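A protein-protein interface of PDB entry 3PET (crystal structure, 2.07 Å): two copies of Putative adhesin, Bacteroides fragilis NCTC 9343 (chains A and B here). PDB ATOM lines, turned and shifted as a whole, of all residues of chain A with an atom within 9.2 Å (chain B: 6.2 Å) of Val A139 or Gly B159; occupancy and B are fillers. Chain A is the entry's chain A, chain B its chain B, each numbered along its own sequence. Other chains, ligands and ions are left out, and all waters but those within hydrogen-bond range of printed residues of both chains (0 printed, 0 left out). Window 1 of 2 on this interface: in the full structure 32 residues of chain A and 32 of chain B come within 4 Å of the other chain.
Of the 15 printed residues of chain B, 9 touch a printed residue of chain A.
Hydrophobic or aromatic side chains of chain B within 4 Å of the printed part of chain A: Val B139, Val B158 and Val B178.
Along chain B the printed residues that touch a printed residue of chain A span positions 139 to 180.
Hydrophobic or aromatic side chains of chain A that line the printed part of chain B: Val A119, Val A139, Val A158 and Val A178.
Along chain A the printed residues that touch a printed residue of chain B span positions 117 to 178.
Gly A138 touches Val B178, but with the chains exchanged Val A178 does not touch Gly B138 (7.5 Å).
Gly A157 touches Val B139, but with the chains exchanged Val A139 does not touch Gly B157 (6.7 Å).
Val A158 touches Val B139, but with the chains exchanged Val A139 does not touch Val B158 (4.1 Å).
Val A158 touches Gly B140, but with the chains exchanged Gly A140 does not touch Val B158 (7.0 Å).
The backbone carbonyl oxygen of Gly A97 is in hydrogen-bond range of the backbone NH of Val A119 (2.9 Å).
O of Val A119 is in hydrogen-bond range of N of Gly A99 (2.9 Å).
O of Ser A116 is in hydrogen-bond range of N of Met A137.
The backbone NH (N) of Gly A120 is in hydrogen-bond range of the backbone carbonyl oxygen (O) of Val A139, 2.9 Å away.
O of Val A158 lies within hydrogen-bond range of N of Gly A140, 2.9 Å away.
N of Val B142 is in hydrogen-bond range of O of Asn B160 (2.9 Å).
Printed residues of chain B within 4 Å of Lys A117: Val B178.
Printed residues of chain B within 4 Å of Gly A118: Val B178 (3.5 Å).
Printed residues of chain B within 4 Å of Gly A138: Val B158 (3.4 Å) and Val B178 (3.7 Å).
Of chain B, only Gly B159 (3.5 Å), Asn B160 (3.7 Å), Val B178 (3.6 Å) and Gly B179 (3.96 Å) come within 4 Å of Val A139.
Of the printed residues of chain B, Gly A157 touches Val B139 and Val B158.
Of the printed residues of chain A, Gly B140 touches Val A158 and Val A178.
Val B158 touches just these residues of chain A: Met A137 (3.4 Å), Gly A138 (3.4 Å), Gly A157 (3.7 Å) and Val A158 (3.6 Å).
Gly B159 touches just these residues of chain A: Val A139 and Val A158.
Asn B160 touches just one residue of chain A: Val A139.
Printed residues of chain A within 4 Å of Val B178: Lys A117 (3.6 Å), Gly A118 (3.5 Å), Gly A138 (3.7 Å) and Val A139 (3.6 Å).
The nearest residue of chain A that does not touch Gly B159 is Gly A138 (5.8 Å).
The nearest printed residue of chain B that does not touch Lys A156 is Val B158 (5.3 Å).
Val B178 touches Gly A118 (CG1 to O, 3.5 Å).
CG1 of Val A119 touches OD2 of Asp B180, at 3.7 Å.
Met A137 touches Val B158 (O to CG1, 3.4 Å).
Val A139 touches Asn B160.
O of Val B178 touches CG2 of Val A139, at 3.6 Å.
Val B139 touches Lys A156 (CG1 to O, 3.4 Å).
Val B139 touches Val A158.
OD1 of Asp B141 touches CG1 of Val A158 (3.6 Å).
CG2 of Val A158 touches O of Val B158, at 3.6 Å.
CA of Gly B140 touches CG2 of Val A178, at 3.9 Å.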
ATOM      1  N   PHE A  95      26.576  23.179 -12.770  1.00  0.00           N
ATOM      2  CA  PHE A  95      26.124  23.429 -11.410  1.00  0.00           C
ATOM      3  C   PHE A  95      27.169  22.978 -10.409  1.00  0.00           C
ATOM      4  O   PHE A  95      27.574  21.819 -10.417  1.00  0.00           O
ATOM      5  CB  PHE A  95      24.753  22.771 -11.131  1.00  0.00           C
ATOM      6  CG  PHE A  95      24.206  23.106  -9.757  1.00  0.00           C
ATOM      7  CD1 PHE A  95      23.574  24.319  -9.519  1.00  0.00           C
ATOM      8  CD2 PHE A  95      24.311  22.201  -8.711  1.00  0.00           C
ATOM      9  CE1 PHE A  95      23.051  24.616  -8.259  1.00  0.00           C
ATOM     10  CE2 PHE A  95      23.816  22.514  -7.442  1.00  0.00           C
ATOM     11  CZ  PHE A  95      23.199  23.722  -7.226  1.00  0.00           C
ATOM     12  N   GLY A  97      26.919  24.150  -6.827  1.00  0.00           N
ATOM     13  CA  GLY A  97      26.448  24.608  -5.527  1.00  0.00           C
ATOM     14  C   GLY A  97      25.665  23.584  -4.740  1.00  0.00           C
ATOM     15  O   GLY A  97      25.887  22.377  -4.869  1.00  0.00           O
ATOM     16  N   VAL A  98      24.755  24.071  -3.896  1.00  0.00           N
ATOM     17  CA  VAL A  98      23.890  23.234  -3.072  1.00  0.00           C
ATOM     18  C   VAL A  98      22.462  23.584  -3.425  1.00  0.00           C
ATOM     19  O   VAL A  98      22.045  24.731  -3.255  1.00  0.00           O
ATOM     20  CB  VAL A  98      24.182  23.390  -1.553  1.00  0.00           C
ATOM     21  CG1 VAL A  98      23.119  22.673  -0.709  1.00  0.00           C
ATOM     22  CG2 VAL A  98      25.586  22.906  -1.201  1.00  0.00           C
ATOM     23  N   GLY A  99      21.735  22.606  -3.957  1.00  0.00           N
ATOM     24  CA  GLY A  99      20.347  22.785  -4.384  1.00  0.00           C
ATOM     25  C   GLY A  99      19.978  21.988  -5.626  1.00  0.00           C
ATOM     26  O   GLY A  99      20.841  21.422  -6.311  1.00  0.00           O
ATOM     27  N   ASP A 100      18.677  21.948  -5.926  1.00  0.00           N
ATOM     28  CA  ASP A 100      18.179  21.208  -7.092  1.00  0.00           C
ATOM     29  C   ASP A 100      18.028  22.103  -8.295  1.00  0.00           C
ATOM     30  O   ASP A 100      17.756  23.298  -8.135  1.00  0.00           O
ATOM     31  CB  ASP A 100      16.832  20.531  -6.768  1.00  0.00           C
ATOM     32  CG  ASP A 100      16.904  19.536  -5.614  1.00  0.00           C
ATOM     33  OD1 ASP A 100      17.955  18.899  -5.445  1.00  0.00           O
ATOM     34  OD2 ASP A 100      15.929  19.434  -4.866  1.00  0.00           O
ATOM     35  N   SER A 116      26.999  18.421 -13.574  1.00  0.00           N
ATOM     36  CA  SER A 116      26.596  18.579 -12.170  1.00  0.00           C
ATOM     37  C   SER A 116      27.749  18.190 -11.264  1.00  0.00           C
ATOM     38  O   SER A 116      28.255  17.062 -11.320  1.00  0.00           O
ATOM     39  CB  SER A 116      25.333  17.789 -11.855  1.00  0.00           C
ATOM     40  OG  SER A 116      25.444  16.422 -12.228  1.00  0.00           O
ATOM     41  N   LYS A 117      28.230  19.171 -10.495  1.00  0.00           N
ATOM     42  CA  LYS A 117      29.387  19.031  -9.616  1.00  0.00           C
ATOM     43  C   LYS A 117      29.057  19.524  -8.214  1.00  0.00           C
ATOM     44  O   LYS A 117      29.955  19.940  -7.481  1.00  0.00           O
ATOM     45  CB  LYS A 117      30.569  19.856 -10.195  1.00  0.00           C
ATOM     46  CG  LYS A 117      30.839  19.684 -11.696  1.00  0.00           C
ATOM     47  CD  LYS A 117      31.217  20.981 -12.422  1.00  0.00           C
ATOM     48  CE  LYS A 117      32.678  21.365 -12.267  1.00  0.00           C
ATOM     49  NZ  LYS A 117      33.570  20.552 -13.138  1.00  0.00           N
ATOM     50  N   GLY A 118      27.772  19.564  -7.874  1.00  0.00           N
ATOM     51  CA  GLY A 118      27.341  20.044  -6.565  1.00  0.00           C
ATOM     52  C   GLY A 118      26.576  19.008  -5.774  1.00  0.00           C
ATOM     53  O   GLY A 118      26.652  17.806  -6.068  1.00  0.00           O
ATOM     54  N   VAL A 119      25.882  19.468  -4.729  1.00  0.00           N
ATOM     55  CA  VAL A 119      25.025  18.619  -3.880  1.00  0.00           C
ATOM     56  C   VAL A 119      23.584  18.966  -4.214  1.00  0.00           C
ATOM     57  O   VAL A 119      23.127  20.074  -3.928  1.00  0.00           O
ATOM     58  CB  VAL A 119      25.327  18.768  -2.362  1.00  0.00           C
ATOM     59  CG1 VAL A 119      24.424  17.857  -1.527  1.00  0.00           C
ATOM     60  CG2 VAL A 119      26.797  18.494  -2.070  1.00  0.00           C
ATOM     61  N   GLY A 120      22.900  18.041  -4.867  1.00  0.00           N
ATOM     62  CA  GLY A 120      21.521  18.267  -5.291  1.00  0.00           C
ATOM     63  C   GLY A 120      21.205  17.540  -6.576  1.00  0.00           C
ATOM     64  O   GLY A 120      22.096  16.962  -7.211  1.00  0.00           O
ATOM     65  N   ASN A 121      19.932  17.519  -6.934  1.00  0.00           N
ATOM     66  CA  ASN A 121      19.439  16.804  -8.120  1.00  0.00           C
ATOM     67  C   ASN A 121      19.273  17.709  -9.318  1.00  0.00           C
ATOM     68  O   ASN A 121      19.231  18.928  -9.176  1.00  0.00           O
ATOM     69  CB  ASN A 121      18.073  16.151  -7.806  1.00  0.00           C
ATOM     70  CG  ASN A 121      18.133  15.155  -6.670  1.00  0.00           C
ATOM     71  OD1 ASN A 121      19.109  14.436  -6.494  1.00  0.00           O
ATOM     72  ND2 ASN A 121      17.100  15.082  -5.866  1.00  0.00           N
ATOM     73  N   VAL A 122      19.168  17.107 -10.500  1.00  0.00           N
ATOM     74  CA  VAL A 122      18.866  17.786 -11.758  1.00  0.00           C
ATOM     75  C   VAL A 122      17.625  17.065 -12.296  1.00  0.00           C
ATOM     76  O   VAL A 122      17.621  15.832 -12.405  1.00  0.00           O
ATOM     77  CB  VAL A 122      20.037  17.844 -12.779  1.00  0.00           C
ATOM     78  CG1 VAL A 122      19.615  18.555 -14.075  1.00  0.00           C
ATOM     79  CG2 VAL A 122      21.253  18.539 -12.181  1.00  0.00           C
ATOM     80  N   SER A 136      27.722  13.662 -14.659  1.00  0.00           N
ATOM     81  CA  SER A 136      27.327  13.837 -13.249  1.00  0.00           C
ATOM     82  C   SER A 136      28.511  13.506 -12.383  1.00  0.00           C
ATOM     83  O   SER A 136      29.086  12.429 -12.501  1.00  0.00           O
ATOM     84  CB  SER A 136      26.089  13.020 -12.886  1.00  0.00           C
ATOM     85  OG  SER A 136      26.297  11.622 -13.053  1.00  0.00           O
ATOM     86  N   MET A 137      28.958  14.499 -11.618  1.00  0.00           N
ATOM     87  CA  MET A 137      30.191  14.390 -10.850  1.00  0.00           C
ATOM     88  C   MET A 137      30.050  14.746  -9.377  1.00  0.00           C
ATOM     89  O   MET A 137      31.038  14.694  -8.669  1.00  0.00           O
ATOM     90  CB  MET A 137      31.236  15.321 -11.475  1.00  0.00           C
ATOM     91  CG  MET A 137      31.692  14.887 -12.869  1.00  0.00           C
ATOM     92  SD  MET A 137      32.731  16.315 -13.677  1.00  0.00           S
ATOM     93  CE  MET A 137      31.274  17.317 -14.374  1.00  0.00           C
ATOM     94  N   GLY A 138      28.853  15.091  -8.923  1.00  0.00           N
ATOM     95  CA  GLY A 138      28.644  15.461  -7.529  1.00  0.00           C
ATOM     96  C   GLY A 138      27.827  14.451  -6.764  1.00  0.00           C
ATOM     97  O   GLY A 138      27.912  13.248  -7.037  1.00  0.00           O
ATOM     98  N   VAL A 139      27.031  14.929  -5.796  1.00  0.00           N
ATOM     99  CA  VAL A 139      26.157  14.063  -5.009  1.00  0.00           C
ATOM    100  C   VAL A 139      24.709  14.400  -5.342  1.00  0.00           C
ATOM    101  O   VAL A 139      24.236  15.491  -5.012  1.00  0.00           O
ATOM    102  CB  VAL A 139      26.428  14.138  -3.488  1.00  0.00           C
ATOM    103  CG1 VAL A 139      25.450  13.234  -2.733  1.00  0.00           C
ATOM    104  CG2 VAL A 139      27.867  13.738  -3.184  1.00  0.00           C
ATOM    105  N   GLY A 140      24.021  13.457  -5.978  1.00  0.00           N
ATOM    106  CA  GLY A 140      22.648  13.682  -6.403  1.00  0.00           C
ATOM    107  C   GLY A 140      22.314  12.949  -7.689  1.00  0.00           C
ATOM    108  O   GLY A 140      23.188  12.375  -8.357  1.00  0.00           O
ATOM    109  N   ASP A 141      21.036  12.963  -8.026  1.00  0.00           N
ATOM    110  CA  ASP A 141      20.493  12.286  -9.211  1.00  0.00           C
ATOM    111  C   ASP A 141      20.258  13.231 -10.366  1.00  0.00           C
ATOM    112  O   ASP A 141      19.951  14.403 -10.148  1.00  0.00           O
ATOM    113  CB  ASP A 141      19.159  11.620  -8.844  1.00  0.00           C
ATOM    114  CG  ASP A 141      19.261  10.489  -7.839  1.00  0.00           C
ATOM    115  OD1 ASP A 141      20.383   9.988  -7.613  1.00  0.00           O
ATOM    116  OD2 ASP A 141      18.216  10.064  -7.323  1.00  0.00           O
ATOM    117  N   VAL A 142      20.376  12.720 -11.604  1.00  0.00           N
ATOM    118  CA  VAL A 142      20.068  13.485 -12.812  1.00  0.00           C
ATOM    119  C   VAL A 142      18.885  12.772 -13.475  1.00  0.00           C
ATOM    120  O   VAL A 142      19.036  11.638 -13.931  1.00  0.00           O
ATOM    121  CB  VAL A 142      21.273  13.689 -13.769  1.00  0.00           C
ATOM    122  CG1 VAL A 142      20.858  14.456 -15.038  1.00  0.00           C
ATOM    123  CG2 VAL A 142      22.400  14.422 -13.059  1.00  0.00           C
ATOM    124  N   LYS A 156      29.874   9.852 -12.582  1.00  0.00           N
ATOM    125  CA  LYS A 156      31.181   9.763 -11.901  1.00  0.00           C
ATOM    126  C   LYS A 156      31.116  10.042 -10.402  1.00  0.00           C
ATOM    127  O   LYS A 156      32.101   9.813  -9.712  1.00  0.00           O
ATOM    128  CB  LYS A 156      32.195  10.742 -12.536  1.00  0.00           C
ATOM    129  CG  LYS A 156      32.514  10.424 -13.991  1.00  0.00           C
ATOM    130  CD  LYS A 156      33.220  11.571 -14.693  1.00  0.00           C
ATOM    131  CE  LYS A 156      33.606  11.152 -16.088  1.00  0.00           C
ATOM    132  NZ  LYS A 156      34.307  12.231 -16.832  1.00  0.00           N
ATOM    133  N   GLY A 157      29.995  10.561  -9.915  1.00  0.00           N
ATOM    134  CA  GLY A 157      29.859  10.882  -8.501  1.00  0.00           C
ATOM    135  C   GLY A 157      29.039   9.852  -7.760  1.00  0.00           C
ATOM    136  O   GLY A 157      29.150   8.644  -8.012  1.00  0.00           O
ATOM    137  N   VAL A 158      28.208  10.321  -6.830  1.00  0.00           N
ATOM    138  CA  VAL A 158      27.325   9.436  -6.062  1.00  0.00           C
ATOM    139  C   VAL A 158      25.881   9.817  -6.423  1.00  0.00           C
ATOM    140  O   VAL A 158      25.461  10.946  -6.170  1.00  0.00           O
ATOM    141  CB  VAL A 158      27.602   9.508  -4.540  1.00  0.00           C
ATOM    142  CG1 VAL A 158      26.630   8.618  -3.765  1.00  0.00           C
ATOM    143  CG2 VAL A 158      29.048   9.113  -4.239  1.00  0.00           C
ATOM    144  N   GLY A 159      25.156   8.884  -7.006  1.00  0.00           N
ATOM    145  CA  GLY A 159      23.790   9.150  -7.454  1.00  0.00           C
ATOM    146  C   GLY A 159      23.486   8.459  -8.774  1.00  0.00           C
ATOM    147  O   GLY A 159      24.368   7.856  -9.406  1.00  0.00           O
ATOM    148  N   ASN A 160      22.228   8.543  -9.189  1.00  0.00           N
ATOM    149  CA  ASN A 160      21.723   7.872 -10.387  1.00  0.00           C
ATOM    150  C   ASN A 160      21.397   8.801 -11.517  1.00  0.00           C
ATOM    151  O   ASN A 160      20.939   9.920 -11.289  1.00  0.00           O
ATOM    152  CB  ASN A 160      20.408   7.120 -10.034  1.00  0.00           C
ATOM    153  CG  ASN A 160      20.577   6.059  -8.978  1.00  0.00           C
ATOM    154  OD1 ASN A 160      21.629   5.466  -8.838  1.00  0.00           O
ATOM    155  ND2 ASN A 160      19.539   5.759  -8.235  1.00  0.00           N
ATOM    156  N   VAL A 178      29.334   5.714  -7.831  1.00  0.00           N
ATOM    157  CA  VAL A 178      28.417   4.837  -7.093  1.00  0.00           C
ATOM    158  C   VAL A 178      27.010   5.217  -7.504  1.00  0.00           C
ATOM    159  O   VAL A 178      26.580   6.340  -7.222  1.00  0.00           O
ATOM    160  CB  VAL A 178      28.639   4.942  -5.561  1.00  0.00           C
ATOM    161  CG1 VAL A 178      27.625   4.090  -4.801  1.00  0.00           C
ATOM    162  CG2 VAL A 178      30.061   4.537  -5.193  1.00  0.00           C
ATOM    163  N   SER B 136      37.739  10.139   3.792  1.00  0.00           N
ATOM    164  CA  SER B 136      37.122   9.681   2.539  1.00  0.00           C
ATOM    165  C   SER B 136      37.713  10.531   1.383  1.00  0.00           C
ATOM    166  O   SER B 136      37.660  11.756   1.435  1.00  0.00           O
ATOM    167  CB  SER B 136      35.592   9.721   2.607  1.00  0.00           C
ATOM    168  OG  SER B 136      35.105  11.038   2.788  1.00  0.00           O
ATOM    169  N   GLY B 138      37.824   9.076  -2.126  1.00  0.00           N
ATOM    170  CA  GLY B 138      37.356   8.524  -3.391  1.00  0.00           C
ATOM    171  C   GLY B 138      35.936   8.932  -3.716  1.00  0.00           C
ATOM    172  O   GLY B 138      35.511  10.053  -3.412  1.00  0.00           O
ATOM    173  N   VAL B 139      35.214   8.037  -4.383  1.00  0.00           N
ATOM    174  CA  VAL B 139      33.825   8.255  -4.776  1.00  0.00           C
ATOM    175  C   VAL B 139      32.956   7.273  -4.022  1.00  0.00           C
ATOM    176  O   VAL B 139      33.068   6.065  -4.220  1.00  0.00           O
ATOM    177  CB  VAL B 139      33.584   8.179  -6.305  1.00  0.00           C
ATOM    178  CG1 VAL B 139      32.105   8.380  -6.606  1.00  0.00           C
ATOM    179  CG2 VAL B 139      34.422   9.231  -7.032  1.00  0.00           C
ATOM    180  N   GLY B 140      32.099   7.802  -3.151  1.00  0.00           N
ATOM    181  CA  GLY B 140      31.228   6.949  -2.366  1.00  0.00           C
ATOM    182  C   GLY B 140      30.889   7.547  -1.033  1.00  0.00           C
ATOM    183  O   GLY B 140      31.496   8.543  -0.615  1.00  0.00           O
ATOM    184  N   ASP B 141      29.899   6.938  -0.374  1.00  0.00           N
ATOM    185  CA  ASP B 141      29.448   7.357   0.937  1.00  0.00           C
ATOM    186  C   ASP B 141      30.059   6.512   2.036  1.00  0.00           C
ATOM    187  O   ASP B 141      30.354   5.331   1.830  1.00  0.00           O
ATOM    188  CB  ASP B 141      27.922   7.236   1.010  1.00  0.00           C
ATOM    189  CG  ASP B 141      27.143   8.185   0.121  1.00  0.00           C
ATOM    190  OD1 ASP B 141      27.750   9.157  -0.396  1.00  0.00           O
ATOM    191  OD2 ASP B 141      25.919   7.992  -0.010  1.00  0.00           O
ATOM    192  N   VAL B 142      30.236   7.102   3.213  1.00  0.00           N
ATOM    193  CA  VAL B 142      30.725   6.373   4.380  1.00  0.00           C
ATOM    194  C   VAL B 142      29.581   6.459   5.390  1.00  0.00           C
ATOM    195  O   VAL B 142      29.256   7.550   5.865  1.00  0.00           O
ATOM    196  CB  VAL B 142      32.096   6.882   4.924  1.00  0.00           C
ATOM    197  CG1 VAL B 142      32.485   6.133   6.215  1.00  0.00           C
ATOM    198  CG2 VAL B 142      33.207   6.754   3.859  1.00  0.00           C
ATOM    199  N   SER B 155      36.072  14.483   4.845  1.00  0.00           N
ATOM    200  CA  SER B 155      35.660  14.119   3.506  1.00  0.00           C
ATOM    201  C   SER B 155      36.416  14.999   2.519  1.00  0.00           C
ATOM    202  O   SER B 155      36.524  16.216   2.733  1.00  0.00           O
ATOM    203  CB  SER B 155      34.146  14.223   3.356  1.00  0.00           C
ATOM    204  OG  SER B 155      33.657  15.522   3.635  1.00  0.00           O
ATOM    205  N   GLY B 157      36.689  13.633  -1.148  1.00  0.00           N
ATOM    206  CA  GLY B 157      36.315  13.198  -2.487  1.00  0.00           C
ATOM    207  C   GLY B 157      34.897  13.591  -2.847  1.00  0.00           C
ATOM    208  O   GLY B 157      34.480  14.725  -2.611  1.00  0.00           O
ATOM    209  N   VAL B 158      34.145  12.657  -3.411  1.00  0.00           N
ATOM    210  CA  VAL B 158      32.754  12.907  -3.791  1.00  0.00           C
ATOM    211  C   VAL B 158      31.917  11.899  -3.025  1.00  0.00           C
ATOM    212  O   VAL B 158      32.119  10.691  -3.176  1.00  0.00           O
ATOM    213  CB  VAL B 158      32.507  12.848  -5.336  1.00  0.00           C
ATOM    214  CG1 VAL B 158      31.015  13.029  -5.666  1.00  0.00           C
ATOM    215  CG2 VAL B 158      33.349  13.899  -6.064  1.00  0.00           C
ATOM    216  N   GLY B 159      30.998  12.401  -2.208  1.00  0.00           N
ATOM    217  CA  GLY B 159      30.139  11.531  -1.416  1.00  0.00           C
ATOM    218  C   GLY B 159      29.876  12.092  -0.041  1.00  0.00           C
ATOM    219  O   GLY B 159      30.492  13.087   0.367  1.00  0.00           O
ATOM    220  N   ASN B 160      28.959  11.441   0.685  1.00  0.00           N
ATOM    221  CA  ASN B 160      28.548  11.860   2.017  1.00  0.00           C
ATOM    222  C   ASN B 160      29.080  10.996   3.120  1.00  0.00           C
ATOM    223  O   ASN B 160      29.199   9.789   2.962  1.00  0.00           O
ATOM    224  CB  ASN B 160      27.025  11.826   2.113  1.00  0.00           C
ATOM    225  CG  ASN B 160      26.310  12.745   1.166  1.00  0.00           C
ATOM    226  OD1 ASN B 160      26.840  13.757   0.709  1.00  0.00           O
ATOM    227  ND2 ASN B 160      25.065  12.428   0.892  1.00  0.00           N
ATOM    228  N   ILE B 161      29.332  11.605   4.273  1.00  0.00           N
ATOM    229  CA  ILE B 161      29.636  10.865   5.495  1.00  0.00           C
ATOM    230  C   ILE B 161      28.326  10.875   6.241  1.00  0.00           C
ATOM    231  O   ILE B 161      27.857  11.936   6.638  1.00  0.00           O
ATOM    232  CB  ILE B 161      30.831  11.366   6.335  1.00  0.00           C
ATOM    233  CG1 ILE B 161      32.155  11.308   5.512  1.00  0.00           C
ATOM    234  CG2 ILE B 161      30.904  10.509   7.643  1.00  0.00           C
ATOM    235  CD1 ILE B 161      33.443  11.702   6.295  1.00  0.00           C
ATOM    236  N   VAL B 178      33.010  17.269  -2.492  1.00  0.00           N
ATOM    237  CA  VAL B 178      31.608  17.497  -2.842  1.00  0.00           C
ATOM    238  C   VAL B 178      30.797  16.505  -2.030  1.00  0.00           C
ATOM    239  O   VAL B 178      30.943  15.304  -2.225  1.00  0.00           O
ATOM    240  CB  VAL B 178      31.355  17.363  -4.370  1.00  0.00           C
ATOM    241  CG1 VAL B 178      29.860  17.519  -4.703  1.00  0.00           C
ATOM    242  CG2 VAL B 178      32.207  18.369  -5.152  1.00  0.00           C
ATOM    243  N   GLY B 179      29.966  17.010  -1.126  1.00  0.00           N
ATOM    244  CA  GLY B 179      29.131  16.148  -0.308  1.00  0.00           C
ATOM    245  C   GLY B 179      28.916  16.699   1.079  1.00  0.00           C
ATOM    246  O   GLY B 179      29.586  17.658   1.480  1.00  0.00           O
ATOM    247  N   ASP B 180      27.991  16.069   1.821  1.00  0.00           N
ATOM    248  CA  ASP B 180      27.639  16.482   3.166  1.00  0.00           C
ATOM    249  C   ASP B 180      28.209  15.588   4.235  1.00  0.00           C
ATOM    250  O   ASP B 180      28.467  14.415   3.987  1.00  0.00           O
ATOM    251  CB  ASP B 180      26.114  16.457   3.308  1.00  0.00           C
ATOM    252  CG  ASP B 180      25.345  17.411   2.398  1.00  0.00           C
ATOM    253  OD1 ASP B 180      25.920  18.451   1.984  1.00  0.00           O
ATOM    254  OD2 ASP B 180      24.175  17.129   2.119  1.00  0.00           O
